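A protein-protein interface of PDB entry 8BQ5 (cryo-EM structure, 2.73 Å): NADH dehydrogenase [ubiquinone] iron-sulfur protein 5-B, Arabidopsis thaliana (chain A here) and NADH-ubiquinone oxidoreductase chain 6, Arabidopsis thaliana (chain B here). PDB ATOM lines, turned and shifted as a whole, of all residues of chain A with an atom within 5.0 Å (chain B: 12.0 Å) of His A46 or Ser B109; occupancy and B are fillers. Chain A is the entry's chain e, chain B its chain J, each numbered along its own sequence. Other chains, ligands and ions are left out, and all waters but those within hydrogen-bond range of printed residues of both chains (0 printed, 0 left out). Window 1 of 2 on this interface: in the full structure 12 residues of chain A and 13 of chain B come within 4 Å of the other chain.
A ring nitrogen (NE2) of His A46 sits at hydrogen-bond distance from the side-chain carboxylate (OE1) of Glu B108 (2.7 Å).
OE1 of Glu A43 is in hydrogen-bond range of N of Ser A48 (3.3 Å).
Ser B109 touches His A46 (OG to ND1, 3.7 Å). Ser A48 touches Glu B108. Ser A48 touches Ile B110 (OG to CD1, 3.3 Å). Phe A51 touches Ile B110. CD1 of Phe A51 touches CD1 of Leu B112, 3.8 Å away.
Leu A42 touches none of the printed residues of chain B. No residue of chain B comes within 4 Å of Glu A43. Leu A45 touches none of the printed residues of chain B. No residue of chain B comes within 4 Å of His A47. Ser A48 touches just these residues of chain B: Glu B108 and Ile B110. Printed residues of chain B within 4 Å of Phe A51: Ile B110 and Leu B112. Of the printed residues of chain A, Ile B110 touches Ser A48 and Phe A51. Of the printed residues of chain A, Glu B108 touches His A46 (2.7 Å) and Ser A48 (3.5 Å). Met B101 touches none of the printed residues of chain A. Leu B113 touches none of the printed residues of chain A. The nearest printed residue of chain A that does not touch Ser B109 is Ser A48 (5.3 Å). The nearest printed residue of chain A that does not touch Glu B108 is Leu A42 (5.6 Å).
Of the 14 printed residues of chain B, 4 touch a printed residue of chain A. Printed residues of chain B that touch a printed residue of chain A: Glu B108, Ser B109, Ile B110 and Leu B112. Hydrophobic or aromatic side chains of chain A that line the printed part of chain B: His A46 and Phe A51. Among the printed residues, 6 pairs touch across the chains. Among the printed residues, no Asp or Glu carboxylate lies within 4 Å of a Lys or Arg side-chain nitrogen of the other chain.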
ATOM      1  N   LEU A  42      -1.854  -4.430   5.046  1.00  0.00           N
ATOM      2  CA  LEU A  42      -2.790  -5.544   5.174  1.00  0.00           C
ATOM      3  C   LEU A  42      -2.308  -6.577   6.190  1.00  0.00           C
ATOM      4  O   LEU A  42      -3.127  -7.181   6.897  1.00  0.00           O
ATOM      5  CB  LEU A  42      -3.035  -6.194   3.812  1.00  0.00           C
ATOM      6  CG  LEU A  42      -3.584  -5.268   2.720  1.00  0.00           C
ATOM      7  CD1 LEU A  42      -3.732  -6.004   1.399  1.00  0.00           C
ATOM      8  CD2 LEU A  42      -4.911  -4.663   3.146  1.00  0.00           C
ATOM      9  N   GLU A  43      -0.993  -6.788   6.287  1.00  0.00           N
ATOM     10  CA  GLU A  43      -0.451  -7.689   7.295  1.00  0.00           C
ATOM     11  C   GLU A  43      -0.697  -7.154   8.697  1.00  0.00           C
ATOM     12  O   GLU A  43      -0.980  -7.924   9.622  1.00  0.00           O
ATOM     13  CB  GLU A  43       1.043  -7.904   7.051  1.00  0.00           C
ATOM     14  CG  GLU A  43       1.717  -8.860   8.021  1.00  0.00           C
ATOM     15  CD  GLU A  43       1.079 -10.234   8.045  1.00  0.00           C
ATOM     16  OE1 GLU A  43       0.521 -10.661   7.014  1.00  0.00           O
ATOM     17  OE2 GLU A  43       1.143 -10.892   9.102  1.00  0.00           O
ATOM     18  N   CYS A  44      -0.580  -5.839   8.880  1.00  0.00           N
ATOM     19  CA  CYS A  44      -0.958  -5.256  10.163  1.00  0.00           C
ATOM     20  C   CYS A  44      -2.435  -5.479  10.450  1.00  0.00           C
ATOM     21  O   CYS A  44      -2.810  -5.765  11.592  1.00  0.00           O
ATOM     22  CB  CYS A  44      -0.638  -3.762  10.193  1.00  0.00           C
ATOM     23  SG  CYS A  44      -1.042  -2.955  11.763  1.00  0.00           S
ATOM     24  N   LEU A  45      -3.284  -5.341   9.430  1.00  0.00           N
ATOM     25  CA  LEU A  45      -4.716  -5.533   9.639  1.00  0.00           C
ATOM     26  C   LEU A  45      -5.038  -6.955  10.082  1.00  0.00           C
ATOM     27  O   LEU A  45      -5.749  -7.153  11.074  1.00  0.00           O
ATOM     28  CB  LEU A  45      -5.493  -5.201   8.367  1.00  0.00           C
ATOM     29  CG  LEU A  45      -5.584  -3.741   7.929  1.00  0.00           C
ATOM     30  CD1 LEU A  45      -6.562  -3.629   6.776  1.00  0.00           C
ATOM     31  CD2 LEU A  45      -6.000  -2.845   9.082  1.00  0.00           C
ATOM     32  N   HIS A  46      -4.531  -7.961   9.366  1.00  0.00           N
ATOM     33  CA  HIS A  46      -5.005  -9.324   9.555  1.00  0.00           C
ATOM     34  C   HIS A  46      -3.976 -10.302  10.108  1.00  0.00           C
ATOM     35  O   HIS A  46      -4.358 -11.426  10.453  1.00  0.00           O
ATOM     36  CB  HIS A  46      -5.553  -9.882   8.232  1.00  0.00           C
ATOM     37  CG  HIS A  46      -6.553  -8.986   7.571  1.00  0.00           C
ATOM     38  ND1 HIS A  46      -7.752  -8.644   8.161  1.00  0.00           N
ATOM     39  CD2 HIS A  46      -6.532  -8.357   6.372  1.00  0.00           C
ATOM     40  CE1 HIS A  46      -8.426  -7.846   7.352  1.00  0.00           C
ATOM     41  NE2 HIS A  46      -7.708  -7.657   6.261  1.00  0.00           N
ATOM     42  N   HIS A  47      -2.699  -9.923  10.198  1.00  0.00           N
ATOM     43  CA  HIS A  47      -1.643 -10.794  10.727  1.00  0.00           C
ATOM     44  C   HIS A  47      -1.575 -12.134   9.999  1.00  0.00           C
ATOM     45  O   HIS A  47      -1.238 -13.156  10.597  1.00  0.00           O
ATOM     46  CB  HIS A  47      -1.812 -11.040  12.229  1.00  0.00           C
ATOM     47  CG  HIS A  47      -2.044  -9.798  13.029  1.00  0.00           C
ATOM     48  ND1 HIS A  47      -1.090  -8.815  13.168  1.00  0.00           N
ATOM     49  CD2 HIS A  47      -3.113  -9.389  13.750  1.00  0.00           C
ATOM     50  CE1 HIS A  47      -1.564  -7.849  13.932  1.00  0.00           C
ATOM     51  NE2 HIS A  47      -2.790  -8.173  14.299  1.00  0.00           N
ATOM     52  N   SER A  48      -1.881 -12.142   8.703  1.00  0.00           N
ATOM     53  CA  SER A  48      -2.060 -13.409   8.002  1.00  0.00           C
ATOM     54  C   SER A  48      -0.744 -14.169   7.869  1.00  0.00           C
ATOM     55  O   SER A  48      -0.684 -15.376   8.134  1.00  0.00           O
ATOM     56  CB  SER A  48      -2.687 -13.160   6.632  1.00  0.00           C
ATOM     57  OG  SER A  48      -2.826 -14.374   5.919  1.00  0.00           O
ATOM     58  N   PHE A  51       0.695 -15.423  11.343  1.00  0.00           N
ATOM     59  CA  PHE A  51      -0.022 -16.598  11.822  1.00  0.00           C
ATOM     60  C   PHE A  51       0.268 -17.814  10.952  1.00  0.00           C
ATOM     61  O   PHE A  51       0.362 -18.933  11.461  1.00  0.00           O
ATOM     62  CB  PHE A  51      -1.524 -16.319  11.875  1.00  0.00           C
ATOM     63  CG  PHE A  51      -1.926 -15.370  12.967  1.00  0.00           C
ATOM     64  CD1 PHE A  51      -1.032 -15.010  13.959  1.00  0.00           C
ATOM     65  CD2 PHE A  51      -3.203 -14.840  13.000  1.00  0.00           C
ATOM     66  CE1 PHE A  51      -1.404 -14.137  14.958  1.00  0.00           C
ATOM     67  CE2 PHE A  51      -3.581 -13.969  13.998  1.00  0.00           C
ATOM     68  CZ  PHE A  51      -2.681 -13.616  14.978  1.00  0.00           C
ATOM     69  N   GLU B 100     -19.863 -20.564   1.511  1.00  0.00           N
ATOM     70  CA  GLU B 100     -19.225 -19.368   0.979  1.00  0.00           C
ATOM     71  C   GLU B 100     -18.964 -18.314   2.051  1.00  0.00           C
ATOM     72  O   GLU B 100     -18.027 -17.519   1.917  1.00  0.00           O
ATOM     73  CB  GLU B 100     -20.081 -18.776  -0.146  1.00  0.00           C
ATOM     74  CG  GLU B 100     -19.444 -17.596  -0.855  1.00  0.00           C
ATOM     75  CD  GLU B 100     -18.334 -18.022  -1.800  1.00  0.00           C
ATOM     76  OE1 GLU B 100     -18.555 -18.955  -2.599  1.00  0.00           O
ATOM     77  OE2 GLU B 100     -17.238 -17.423  -1.745  1.00  0.00           O
ATOM     78  N   MET B 101     -19.733 -18.314   3.145  1.00  0.00           N
ATOM     79  CA  MET B 101     -19.836 -17.132   3.980  1.00  0.00           C
ATOM     80  C   MET B 101     -19.377 -17.327   5.420  1.00  0.00           C
ATOM     81  O   MET B 101     -18.963 -16.349   6.049  1.00  0.00           O
ATOM     82  CB  MET B 101     -21.291 -16.639   3.959  1.00  0.00           C
ATOM     83  CG  MET B 101     -21.447 -15.167   4.175  1.00  0.00           C
ATOM     84  SD  MET B 101     -20.960 -14.144   2.779  1.00  0.00           S
ATOM     85  CE  MET B 101     -21.523 -15.147   1.413  1.00  0.00           C
ATOM     86  N   PHE B 102     -19.437 -18.548   5.964  1.00  0.00           N
ATOM     87  CA  PHE B 102     -18.826 -18.807   7.264  1.00  0.00           C
ATOM     88  C   PHE B 102     -17.310 -18.926   7.195  1.00  0.00           C
ATOM     89  O   PHE B 102     -16.652 -18.875   8.239  1.00  0.00           O
ATOM     90  CB  PHE B 102     -19.401 -20.078   7.898  1.00  0.00           C
ATOM     91  CG  PHE B 102     -20.822 -19.946   8.363  1.00  0.00           C
ATOM     92  CD1 PHE B 102     -21.119 -19.988   9.713  1.00  0.00           C
ATOM     93  CD2 PHE B 102     -21.856 -19.771   7.467  1.00  0.00           C
ATOM     94  CE1 PHE B 102     -22.420 -19.869  10.156  1.00  0.00           C
ATOM     95  CE2 PHE B 102     -23.161 -19.655   7.901  1.00  0.00           C
ATOM     96  CZ  PHE B 102     -23.441 -19.701   9.249  1.00  0.00           C
ATOM     97  N   PHE B 103     -16.744 -19.091   6.001  1.00  0.00           N
ATOM     98  CA  PHE B 103     -15.299 -19.172   5.832  1.00  0.00           C
ATOM     99  C   PHE B 103     -14.756 -18.029   4.987  1.00  0.00           C
ATOM    100  O   PHE B 103     -13.742 -18.203   4.299  1.00  0.00           O
ATOM    101  CB  PHE B 103     -14.914 -20.524   5.224  1.00  0.00           C
ATOM    102  CG  PHE B 103     -15.665 -21.681   5.817  1.00  0.00           C
ATOM    103  CD1 PHE B 103     -15.355 -22.148   7.084  1.00  0.00           C
ATOM    104  CD2 PHE B 103     -16.694 -22.287   5.120  1.00  0.00           C
ATOM    105  CE1 PHE B 103     -16.051 -23.205   7.638  1.00  0.00           C
ATOM    106  CE2 PHE B 103     -17.394 -23.343   5.670  1.00  0.00           C
ATOM    107  CZ  PHE B 103     -17.071 -23.801   6.931  1.00  0.00           C
ATOM    108  N   ILE B 104     -15.400 -16.861   5.027  1.00  0.00           N
ATOM    109  CA  ILE B 104     -14.964 -15.743   4.200  1.00  0.00           C
ATOM    110  C   ILE B 104     -13.723 -15.088   4.790  1.00  0.00           C
ATOM    111  O   ILE B 104     -12.936 -14.470   4.064  1.00  0.00           O
ATOM    112  CB  ILE B 104     -16.124 -14.747   4.028  1.00  0.00           C
ATOM    113  CG1 ILE B 104     -15.799 -13.695   2.975  1.00  0.00           C
ATOM    114  CG2 ILE B 104     -16.367 -14.030   5.317  1.00  0.00           C
ATOM    115  CD1 ILE B 104     -16.754 -12.569   2.961  1.00  0.00           C
ATOM    116  N   LEU B 105     -13.519 -15.214   6.100  1.00  0.00           N
ATOM    117  CA  LEU B 105     -12.349 -14.633   6.741  1.00  0.00           C
ATOM    118  C   LEU B 105     -11.172 -15.596   6.820  1.00  0.00           C
ATOM    119  O   LEU B 105     -10.070 -15.163   7.166  1.00  0.00           O
ATOM    120  CB  LEU B 105     -12.701 -14.145   8.151  1.00  0.00           C
ATOM    121  CG  LEU B 105     -13.827 -13.120   8.319  1.00  0.00           C
ATOM    122  CD1 LEU B 105     -13.782 -12.501   9.707  1.00  0.00           C
ATOM    123  CD2 LEU B 105     -13.740 -12.041   7.256  1.00  0.00           C
ATOM    124  N   ASP B 106     -11.368 -16.877   6.496  1.00  0.00           N
ATOM    125  CA  ASP B 106     -10.318 -17.865   6.728  1.00  0.00           C
ATOM    126  C   ASP B 106      -9.087 -17.592   5.872  1.00  0.00           C
ATOM    127  O   ASP B 106      -7.953 -17.688   6.357  1.00  0.00           O
ATOM    128  CB  ASP B 106     -10.860 -19.270   6.475  1.00  0.00           C
ATOM    129  CG  ASP B 106     -11.847 -19.707   7.539  1.00  0.00           C
ATOM    130  OD1 ASP B 106     -12.700 -18.883   7.927  1.00  0.00           O
ATOM    131  OD2 ASP B 106     -11.773 -20.869   7.990  1.00  0.00           O
ATOM    132  N   ASN B 107      -9.284 -17.248   4.600  1.00  0.00           N
ATOM    133  CA  ASN B 107      -8.148 -16.942   3.738  1.00  0.00           C
ATOM    134  C   ASN B 107      -7.507 -15.607   4.090  1.00  0.00           C
ATOM    135  O   ASN B 107      -6.279 -15.477   4.020  1.00  0.00           O
ATOM    136  CB  ASN B 107      -8.582 -16.946   2.273  1.00  0.00           C
ATOM    137  CG  ASN B 107      -8.886 -18.338   1.762  1.00  0.00           C
ATOM    138  OD1 ASN B 107      -8.401 -19.330   2.305  1.00  0.00           O
ATOM    139  ND2 ASN B 107      -9.695 -18.421   0.712  1.00  0.00           N
ATOM    140  N   GLU B 108      -8.310 -14.613   4.466  1.00  0.00           N
ATOM    141  CA  GLU B 108      -7.765 -13.314   4.841  1.00  0.00           C
ATOM    142  C   GLU B 108      -7.248 -13.314   6.274  1.00  0.00           C
ATOM    143  O   GLU B 108      -6.182 -12.756   6.551  1.00  0.00           O
ATOM    144  CB  GLU B 108      -8.829 -12.235   4.655  1.00  0.00           C
ATOM    145  CG  GLU B 108      -8.329 -10.820   4.846  1.00  0.00           C
ATOM    146  CD  GLU B 108      -9.122  -9.819   4.032  1.00  0.00           C
ATOM    147  OE1 GLU B 108      -8.693  -8.651   3.938  1.00  0.00           O
ATOM    148  OE2 GLU B 108     -10.175 -10.205   3.484  1.00  0.00           O
ATOM    149  N   SER B 109      -7.983 -13.934   7.189  1.00  0.00           N
ATOM    150  CA  SER B 109      -7.612 -13.989   8.601  1.00  0.00           C
ATOM    151  C   SER B 109      -7.386 -15.453   8.961  1.00  0.00           C
ATOM    152  O   SER B 109      -8.287 -16.139   9.447  1.00  0.00           O
ATOM    153  CB  SER B 109      -8.689 -13.357   9.470  1.00  0.00           C
ATOM    154  OG  SER B 109      -8.514 -11.955   9.551  1.00  0.00           O
ATOM    155  N   ILE B 110      -6.172 -15.924   8.720  1.00  0.00           N
ATOM    156  CA  ILE B 110      -5.816 -17.307   9.037  1.00  0.00           C
ATOM    157  C   ILE B 110      -5.662 -17.438  10.549  1.00  0.00           C
ATOM    158  O   ILE B 110      -4.900 -16.669  11.155  1.00  0.00           O
ATOM    159  CB  ILE B 110      -4.539 -17.703   8.312  1.00  0.00           C
ATOM    160  CG1 ILE B 110      -4.728 -17.478   6.815  1.00  0.00           C
ATOM    161  CG2 ILE B 110      -4.190 -19.159   8.580  1.00  0.00           C
ATOM    162  CD1 ILE B 110      -3.480 -17.630   6.025  1.00  0.00           C
ATOM    163  N   PRO B 111      -6.370 -18.365  11.187  1.00  0.00           N
ATOM    164  CA  PRO B 111      -6.309 -18.465  12.648  1.00  0.00           C
ATOM    165  C   PRO B 111      -4.952 -18.944  13.138  1.00  0.00           C
ATOM    166  O   PRO B 111      -4.233 -19.676  12.456  1.00  0.00           O
ATOM    167  CB  PRO B 111      -7.407 -19.480  12.980  1.00  0.00           C
ATOM    168  CG  PRO B 111      -7.558 -20.289  11.743  1.00  0.00           C
ATOM    169  CD  PRO B 111      -7.274 -19.365  10.596  1.00  0.00           C
ATOM    170  N   LEU B 112      -4.611 -18.513  14.348  1.00  0.00           N
ATOM    171  CA  LEU B 112      -3.391 -18.945  15.019  1.00  0.00           C
ATOM    172  C   LEU B 112      -3.706 -20.208  15.812  1.00  0.00           C
ATOM    173  O   LEU B 112      -4.475 -20.166  16.778  1.00  0.00           O
ATOM    174  CB  LEU B 112      -2.860 -17.837  15.923  1.00  0.00           C
ATOM    175  CG  LEU B 112      -1.559 -18.099  16.679  1.00  0.00           C
ATOM    176  CD1 LEU B 112      -0.415 -18.331  15.710  1.00  0.00           C
ATOM    177  CD2 LEU B 112      -1.254 -16.933  17.602  1.00  0.00           C
ATOM    178  N   LEU B 113      -3.128 -21.328  15.397  1.00  0.00           N
ATOM    179  CA  LEU B 113      -3.365 -22.589  16.088  1.00  0.00           C
ATOM    180  C   LEU B 113      -2.744 -22.543  17.480  1.00  0.00           C
ATOM    181  O   LEU B 113      -1.625 -22.042  17.639  1.00  0.00           O
ATOM    182  CB  LEU B 113      -2.798 -23.753  15.284  1.00  0.00           C
ATOM    183  CG  LEU B 113      -3.276 -23.781  13.833  1.00  0.00           C
ATOM    184  CD1 LEU B 113      -2.670 -24.936  13.065  1.00  0.00           C
ATOM    185  CD2 LEU B 113      -4.792 -23.848  13.790  1.00  0.00           C
